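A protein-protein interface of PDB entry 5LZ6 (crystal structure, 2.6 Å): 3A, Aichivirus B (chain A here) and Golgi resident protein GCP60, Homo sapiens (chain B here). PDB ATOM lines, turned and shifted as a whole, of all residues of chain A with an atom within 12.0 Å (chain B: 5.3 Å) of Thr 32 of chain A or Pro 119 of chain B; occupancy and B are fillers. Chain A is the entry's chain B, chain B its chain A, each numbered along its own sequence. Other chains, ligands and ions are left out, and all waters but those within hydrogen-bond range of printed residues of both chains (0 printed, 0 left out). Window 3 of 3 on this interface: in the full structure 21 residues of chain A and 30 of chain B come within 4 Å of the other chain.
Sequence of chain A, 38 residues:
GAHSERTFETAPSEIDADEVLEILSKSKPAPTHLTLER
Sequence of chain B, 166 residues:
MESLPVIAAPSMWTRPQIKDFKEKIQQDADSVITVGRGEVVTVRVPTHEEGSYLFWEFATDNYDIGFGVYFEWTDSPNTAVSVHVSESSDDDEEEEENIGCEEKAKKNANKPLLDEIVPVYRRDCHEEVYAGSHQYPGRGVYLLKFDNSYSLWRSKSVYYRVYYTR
The backbone carbonyl oxygen (O) of Met 12 of chain B sits at hydrogen-bond distance from the backbone NH (N) of Ala 30 of chain A (2.6 Å). The guanidinium group of Arg 123 of chain B sits at hydrogen-bond distance from the backbone carbonyl oxygen of Pro 31 of chain A. NH2 of Arg 123 of chain B is in hydrogen-bond range of O of Thr 32 of chain A (3.4 Å).
Printed residues of chain A that touch a printed residue of chain B: Pro 29, Ala 30, Pro 31, Thr 32 and Leu 34. Printed residues of chain B that touch a printed residue of chain A: Pro 10, Met 12, Val 118, Pro 119, Tyr 121 and Arg 123. Hydrophobic or aromatic side chains of chain B within 4 Å of the printed part of chain A: Met 12, Val 118, Pro 119 and Tyr 121. Along chain B the printed residues that touch a printed residue of chain A span positions 10 to 123. Among the printed residues, 10 pairs touch across the chains. Among the printed residues, no Asp or Glu carboxylate lies within 4 Å of a Lys or Arg side-chain nitrogen of the other chain.
Among the printed residues, merely in contact across the chains: Leu 34 of chain A with Tyr 121 of chain B (3.4 Å), Pro 29 of chain A with Met 12 of chain B (3.5 Å), Thr 32 of chain A with Pro 10 of chain B (3.5 Å), Thr 32 of chain A with Pro 119 of chain B (3.7 Å), Thr 32 of chain A with Val 118 of chain B (3.8 Å), Thr 32 of chain A with Met 12 of chain B (3.8 Å) and Leu 34 of chain A with Arg 123 of chain B (3.9 Å).
The guanidinium group (NH1) of Arg 123 of chain B is in hydrogen-bond range of the side-chain sulfur (SD) of Met 12 of chain B (3.5 Å). The backbone NH of Phe 67 of chain B sits at hydrogen-bond distance from the backbone carbonyl oxygen of Tyr 121 of chain B. O of Val 118 of chain B is in hydrogen-bond range of N of Val 69 of chain B (2.9 Å). The backbone carbonyl oxygen (O) of Pro 119 of chain B lies within hydrogen-bond range of the guanidinium group (NH2) of Arg 123 of chain B, at 3.2 Å. The backbone carbonyl oxygen (O) of Tyr 121 of chain B sits at hydrogen-bond distance from the guanidinium group (NE) of Arg 123 of chain B, 3.2 Å away. A ring nitrogen (ND1) of His 33 of chain A sits at hydrogen-bond distance from the side-chain hydroxyl (OG1) of Thr 32 of chain A.
Lys 28 of chain A touches none of the printed residues of chain B. Printed residues of chain B within 4 Å of Pro 29 of chain A: Met 12. Of chain B, only Pro 10, Met 12, Val 118, Pro 119 and Arg 123 come within 4 Å of Thr 32 of chain A. Of chain A, only Thr 32 (3.5 Å) comes within 4 Å of Pro 10 of chain B. No residue of chain A comes within 4 Å of Ser 11 of chain B. Printed residues of chain A within 4 Å of Met 12 of chain B: Pro 29 (3.5 Å), Ala 30 (2.6 Å) and Thr 32 (3.8 Å). Val 69 of chain B touches none of the printed residues of chain A. No residue of chain A comes within 4 Å of Glu 116 of chain B. Ile 117 of chain B touches none of the printed residues of chain A. Pro 119 of chain B touches one residue of chain A. Val 120 of chain B touches none of the printed residues of chain A. The nearest residue of chain B that does not touch Thr 32 of chain A is Ser 11 of chain B (4.1 Å). The nearest residue of chain A that does not touch Pro 119 of chain B is His 33 of chain A (4.1 Å). The nearest printed residue of chain A that does not touch Arg 123 of chain B is His 33 of chain A (5.4 Å).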
ATOM      1  N   LEU A  24      23.397 -16.013  22.303  1.00  0.00           N
ATOM      2  CA  LEU A  24      22.472 -15.519  23.317  1.00  0.00           C
ATOM      3  C   LEU A  24      22.157 -14.031  23.161  1.00  0.00           C
ATOM      4  O   LEU A  24      21.159 -13.547  23.695  1.00  0.00           O
ATOM      5  CB  LEU A  24      23.036 -15.786  24.715  1.00  0.00           C
ATOM      6  CG  LEU A  24      23.198 -17.260  25.105  1.00  0.00           C
ATOM      7  CD1 LEU A  24      23.837 -17.379  26.478  1.00  0.00           C
ATOM      8  CD2 LEU A  24      21.867 -18.001  25.080  1.00  0.00           C
ATOM      9  N   LYS A  28      16.057 -14.898  23.600  1.00  0.00           N
ATOM     10  CA  LYS A  28      15.322 -14.539  24.809  1.00  0.00           C
ATOM     11  C   LYS A  28      14.939 -15.807  25.576  1.00  0.00           C
ATOM     12  O   LYS A  28      14.814 -16.875  24.978  1.00  0.00           O
ATOM     13  CB  LYS A  28      14.074 -13.722  24.466  1.00  0.00           C
ATOM     14  CG  LYS A  28      13.152 -14.379  23.452  1.00  0.00           C
ATOM     15  CD  LYS A  28      11.961 -13.487  23.131  1.00  0.00           C
ATOM     16  CE  LYS A  28      11.083 -14.088  22.041  1.00  0.00           C
ATOM     17  NZ  LYS A  28      10.437 -15.364  22.464  1.00  0.00           N
ATOM     18  N   PRO A  29      14.754 -15.695  26.903  1.00  0.00           N
ATOM     19  CA  PRO A  29      14.453 -16.868  27.736  1.00  0.00           C
ATOM     20  C   PRO A  29      13.222 -17.644  27.282  1.00  0.00           C
ATOM     21  O   PRO A  29      12.258 -17.043  26.805  1.00  0.00           O
ATOM     22  CB  PRO A  29      14.215 -16.264  29.123  1.00  0.00           C
ATOM     23  CG  PRO A  29      14.951 -14.982  29.113  1.00  0.00           C
ATOM     24  CD  PRO A  29      14.852 -14.465  27.710  1.00  0.00           C
ATOM     25  N   ALA A  30      13.270 -18.964  27.437  1.00  0.00           N
ATOM     26  CA  ALA A  30      12.141 -19.834  27.129  1.00  0.00           C
ATOM     27  C   ALA A  30      11.850 -20.741  28.319  1.00  0.00           C
ATOM     28  O   ALA A  30      12.741 -21.002  29.129  1.00  0.00           O
ATOM     29  CB  ALA A  30      12.425 -20.659  25.888  1.00  0.00           C
ATOM     30  N   PRO A  31      10.600 -21.221  28.438  1.00  0.00           N
ATOM     31  CA  PRO A  31      10.270 -22.134  29.539  1.00  0.00           C
ATOM     32  C   PRO A  31      11.056 -23.440  29.477  1.00  0.00           C
ATOM     33  O   PRO A  31      11.200 -24.024  28.401  1.00  0.00           O
ATOM     34  CB  PRO A  31       8.772 -22.395  29.346  1.00  0.00           C
ATOM     35  CG  PRO A  31       8.280 -21.263  28.525  1.00  0.00           C
ATOM     36  CD  PRO A  31       9.416 -20.889  27.629  1.00  0.00           C
ATOM     37  N   THR A  32      11.555 -23.886  30.625  1.00  0.00           N
ATOM     38  CA  THR A  32      12.291 -25.142  30.712  1.00  0.00           C
ATOM     39  C   THR A  32      11.369 -26.300  31.079  1.00  0.00           C
ATOM     40  O   THR A  32      11.399 -27.355  30.447  1.00  0.00           O
ATOM     41  CB  THR A  32      13.420 -25.065  31.760  1.00  0.00           C
ATOM     42  OG1 THR A  32      12.877 -24.664  33.024  1.00  0.00           O
ATOM     43  CG2 THR A  32      14.491 -24.074  31.335  1.00  0.00           C
ATOM     44  N   HIS A  33      10.546 -26.083  32.100  1.00  0.00           N
ATOM     45  CA  HIS A  33       9.765 -27.150  32.718  1.00  0.00           C
ATOM     46  C   HIS A  33       8.269 -27.024  32.456  1.00  0.00           C
ATOM     47  O   HIS A  33       7.482 -27.831  32.953  1.00  0.00           O
ATOM     48  CB  HIS A  33      10.013 -27.158  34.225  1.00  0.00           C
ATOM     49  CG  HIS A  33       9.624 -25.880  34.900  1.00  0.00           C
ATOM     50  ND1 HIS A  33      10.407 -24.746  34.854  1.00  0.00           N
ATOM     51  CD2 HIS A  33       8.532 -25.553  35.630  1.00  0.00           C
ATOM     52  CE1 HIS A  33       9.816 -23.777  35.529  1.00  0.00           C
ATOM     53  NE2 HIS A  33       8.677 -24.241  36.011  1.00  0.00           N
ATOM     54  N   LEU A  34       7.883 -26.014  31.682  1.00  0.00           N
ATOM     55  CA  LEU A  34       6.481 -25.788  31.345  1.00  0.00           C
ATOM     56  C   LEU A  34       5.634 -25.601  32.605  1.00  0.00           C
ATOM     57  O   LEU A  34       4.948 -26.521  33.056  1.00  0.00           O
ATOM     58  CB  LEU A  34       5.935 -26.950  30.505  1.00  0.00           C
ATOM     59  CG  LEU A  34       6.683 -27.333  29.217  1.00  0.00           C
ATOM     60  CD1 LEU A  34       7.251 -26.106  28.507  1.00  0.00           C
ATOM     61  CD2 LEU A  34       7.789 -28.360  29.474  1.00  0.00           C
ATOM     62  N   PRO B  10      18.386 -26.293  34.423  1.00  0.00           N
ATOM     63  CA  PRO B  10      18.843 -25.903  33.088  1.00  0.00           C
ATOM     64  C   PRO B  10      18.296 -24.539  32.682  1.00  0.00           C
ATOM     65  O   PRO B  10      17.394 -24.028  33.342  1.00  0.00           O
ATOM     66  CB  PRO B  10      18.282 -27.012  32.197  1.00  0.00           C
ATOM     67  CG  PRO B  10      17.007 -27.390  32.868  1.00  0.00           C
ATOM     68  CD  PRO B  10      17.235 -27.211  34.355  1.00  0.00           C
ATOM     69  N   SER B  11      18.845 -23.967  31.616  1.00  0.00           N
ATOM     70  CA  SER B  11      18.324 -22.734  31.038  1.00  0.00           C
ATOM     71  C   SER B  11      18.010 -22.957  29.566  1.00  0.00           C
ATOM     72  O   SER B  11      18.653 -23.774  28.907  1.00  0.00           O
ATOM     73  CB  SER B  11      19.323 -21.589  31.208  1.00  0.00           C
ATOM     74  OG  SER B  11      19.387 -21.168  32.559  1.00  0.00           O
ATOM     75  N   MET B  12      17.016 -22.235  29.058  1.00  0.00           N
ATOM     76  CA  MET B  12      16.591 -22.390  27.671  1.00  0.00           C
ATOM     77  C   MET B  12      16.211 -21.053  27.052  1.00  0.00           C
ATOM     78  O   MET B  12      15.581 -20.213  27.695  1.00  0.00           O
ATOM     79  CB  MET B  12      15.412 -23.354  27.582  1.00  0.00           C
ATOM     80  CG  MET B  12      15.502 -24.339  26.422  1.00  0.00           C
ATOM     81  SD  MET B  12      14.313 -25.693  26.522  1.00  0.00           S
ATOM     82  CE  MET B  12      14.757 -26.411  28.103  1.00  0.00           C
ATOM     83  N   PHE B  67      10.729 -32.244  22.778  1.00  0.00           N
ATOM     84  CA  PHE B  67      12.124 -32.171  23.193  1.00  0.00           C
ATOM     85  C   PHE B  67      12.266 -32.266  24.705  1.00  0.00           C
ATOM     86  O   PHE B  67      11.461 -31.712  25.451  1.00  0.00           O
ATOM     87  CB  PHE B  67      12.772 -30.876  22.704  1.00  0.00           C
ATOM     88  CG  PHE B  67      14.184 -30.699  23.183  1.00  0.00           C
ATOM     89  CD1 PHE B  67      15.241 -31.266  22.491  1.00  0.00           C
ATOM     90  CD2 PHE B  67      14.452 -29.973  24.333  1.00  0.00           C
ATOM     91  CE1 PHE B  67      16.542 -31.108  22.933  1.00  0.00           C
ATOM     92  CE2 PHE B  67      15.750 -29.812  24.780  1.00  0.00           C
ATOM     93  CZ  PHE B  67      16.797 -30.380  24.080  1.00  0.00           C
ATOM     94  N   GLY B  68      13.305 -32.969  25.141  1.00  0.00           N
ATOM     95  CA  GLY B  68      13.639 -33.073  26.548  1.00  0.00           C
ATOM     96  C   GLY B  68      15.078 -33.514  26.714  1.00  0.00           C
ATOM     97  O   GLY B  68      15.731 -33.893  25.742  1.00  0.00           O
ATOM     98  N   VAL B  69      15.573 -33.460  27.949  1.00  0.00           N
ATOM     99  CA  VAL B  69      16.954 -33.821  28.247  1.00  0.00           C
ATOM    100  C   VAL B  69      17.020 -34.637  29.529  1.00  0.00           C
ATOM    101  O   VAL B  69      16.354 -34.320  30.514  1.00  0.00           O
ATOM    102  CB  VAL B  69      17.858 -32.570  28.394  1.00  0.00           C
ATOM    103  CG1 VAL B  69      19.306 -32.973  28.687  1.00  0.00           C
ATOM    104  CG2 VAL B  69      17.795 -31.714  27.143  1.00  0.00           C
ATOM    105  N   GLU B 116      16.102 -36.389  35.361  1.00  0.00           N
ATOM    106  CA  GLU B 116      15.325 -35.562  34.444  1.00  0.00           C
ATOM    107  C   GLU B 116      15.774 -34.105  34.523  1.00  0.00           C
ATOM    108  O   GLU B 116      15.600 -33.447  35.549  1.00  0.00           O
ATOM    109  CB  GLU B 116      13.831 -35.666  34.752  1.00  0.00           C
ATOM    110  CG  GLU B 116      12.952 -34.970  33.727  1.00  0.00           C
ATOM    111  CD  GLU B 116      11.482 -34.993  34.095  1.00  0.00           C
ATOM    112  OE1 GLU B 116      11.166 -34.908  35.300  1.00  0.00           O
ATOM    113  OE2 GLU B 116      10.641 -35.097  33.176  1.00  0.00           O
ATOM    114  N   ILE B 117      16.356 -33.614  33.433  1.00  0.00           N
ATOM    115  CA  ILE B 117      16.854 -32.245  33.363  1.00  0.00           C
ATOM    116  C   ILE B 117      15.824 -31.312  32.732  1.00  0.00           C
ATOM    117  O   ILE B 117      15.370 -30.356  33.362  1.00  0.00           O
ATOM    118  CB  ILE B 117      18.155 -32.178  32.549  1.00  0.00           C
ATOM    119  CG1 ILE B 117      19.176 -33.186  33.087  1.00  0.00           C
ATOM    120  CG2 ILE B 117      18.735 -30.770  32.562  1.00  0.00           C
ATOM    121  CD1 ILE B 117      19.406 -33.118  34.594  1.00  0.00           C
ATOM    122  N   VAL B 118      15.482 -31.587  31.476  1.00  0.00           N
ATOM    123  CA  VAL B 118      14.428 -30.858  30.778  1.00  0.00           C
ATOM    124  C   VAL B 118      13.267 -31.802  30.481  1.00  0.00           C
ATOM    125  O   VAL B 118      13.410 -32.717  29.668  1.00  0.00           O
ATOM    126  CB  VAL B 118      14.947 -30.235  29.466  1.00  0.00           C
ATOM    127  CG1 VAL B 118      13.797 -29.673  28.637  1.00  0.00           C
ATOM    128  CG2 VAL B 118      15.974 -29.149  29.771  1.00  0.00           C
ATOM    129  N   PRO B 119      12.111 -31.591  31.138  1.00  0.00           N
ATOM    130  CA  PRO B 119      10.965 -32.462  30.850  1.00  0.00           C
ATOM    131  C   PRO B 119      10.552 -32.411  29.383  1.00  0.00           C
ATOM    132  O   PRO B 119      10.647 -31.360  28.749  1.00  0.00           O
ATOM    133  CB  PRO B 119       9.859 -31.901  31.749  1.00  0.00           C
ATOM    134  CG  PRO B 119      10.575 -31.191  32.840  1.00  0.00           C
ATOM    135  CD  PRO B 119      11.801 -30.617  32.198  1.00  0.00           C
ATOM    136  N   VAL B 120      10.100 -33.543  28.857  1.00  0.00           N
ATOM    137  CA  VAL B 120       9.753 -33.647  27.446  1.00  0.00           C
ATOM    138  C   VAL B 120       8.413 -32.983  27.152  1.00  0.00           C
ATOM    139  O   VAL B 120       7.377 -33.390  27.674  1.00  0.00           O
ATOM    140  CB  VAL B 120       9.699 -35.120  26.986  1.00  0.00           C
ATOM    141  CG1 VAL B 120       9.395 -35.214  25.492  1.00  0.00           C
ATOM    142  CG2 VAL B 120      11.012 -35.815  27.290  1.00  0.00           C
ATOM    143  N   TYR B 121       8.450 -31.954  26.311  1.00  0.00           N
ATOM    144  CA  TYR B 121       7.241 -31.296  25.835  1.00  0.00           C
ATOM    145  C   TYR B 121       7.461 -30.813  24.408  1.00  0.00           C
ATOM    146  O   TYR B 121       8.600 -30.635  23.974  1.00  0.00           O
ATOM    147  CB  TYR B 121       6.854 -30.127  26.747  1.00  0.00           C
ATOM    148  N   ARG B 123       7.846 -28.358  21.417  1.00  0.00           N
ATOM    149  CA  ARG B 123       8.367 -27.001  21.267  1.00  0.00           C
ATOM    150  C   ARG B 123       8.140 -26.491  19.852  1.00  0.00           C
ATOM    151  O   ARG B 123       8.336 -27.225  18.885  1.00  0.00           O
ATOM    152  CB  ARG B 123       9.866 -26.949  21.577  1.00  0.00           C
ATOM    153  CG  ARG B 123      10.312 -27.782  22.766  1.00  0.00           C
ATOM    154  CD  ARG B 123       9.769 -27.246  24.075  1.00  0.00           C
ATOM    155  NE  ARG B 123      10.146 -28.110  25.194  1.00  0.00           N
ATOM    156  CZ  ARG B 123      10.668 -27.692  26.346  1.00  0.00           C
ATOM    157  NH1 ARG B 123      10.887 -26.400  26.574  1.00  0.00           N
ATOM    158  NH2 ARG B 123      10.971 -28.579  27.283  1.00  0.00           N
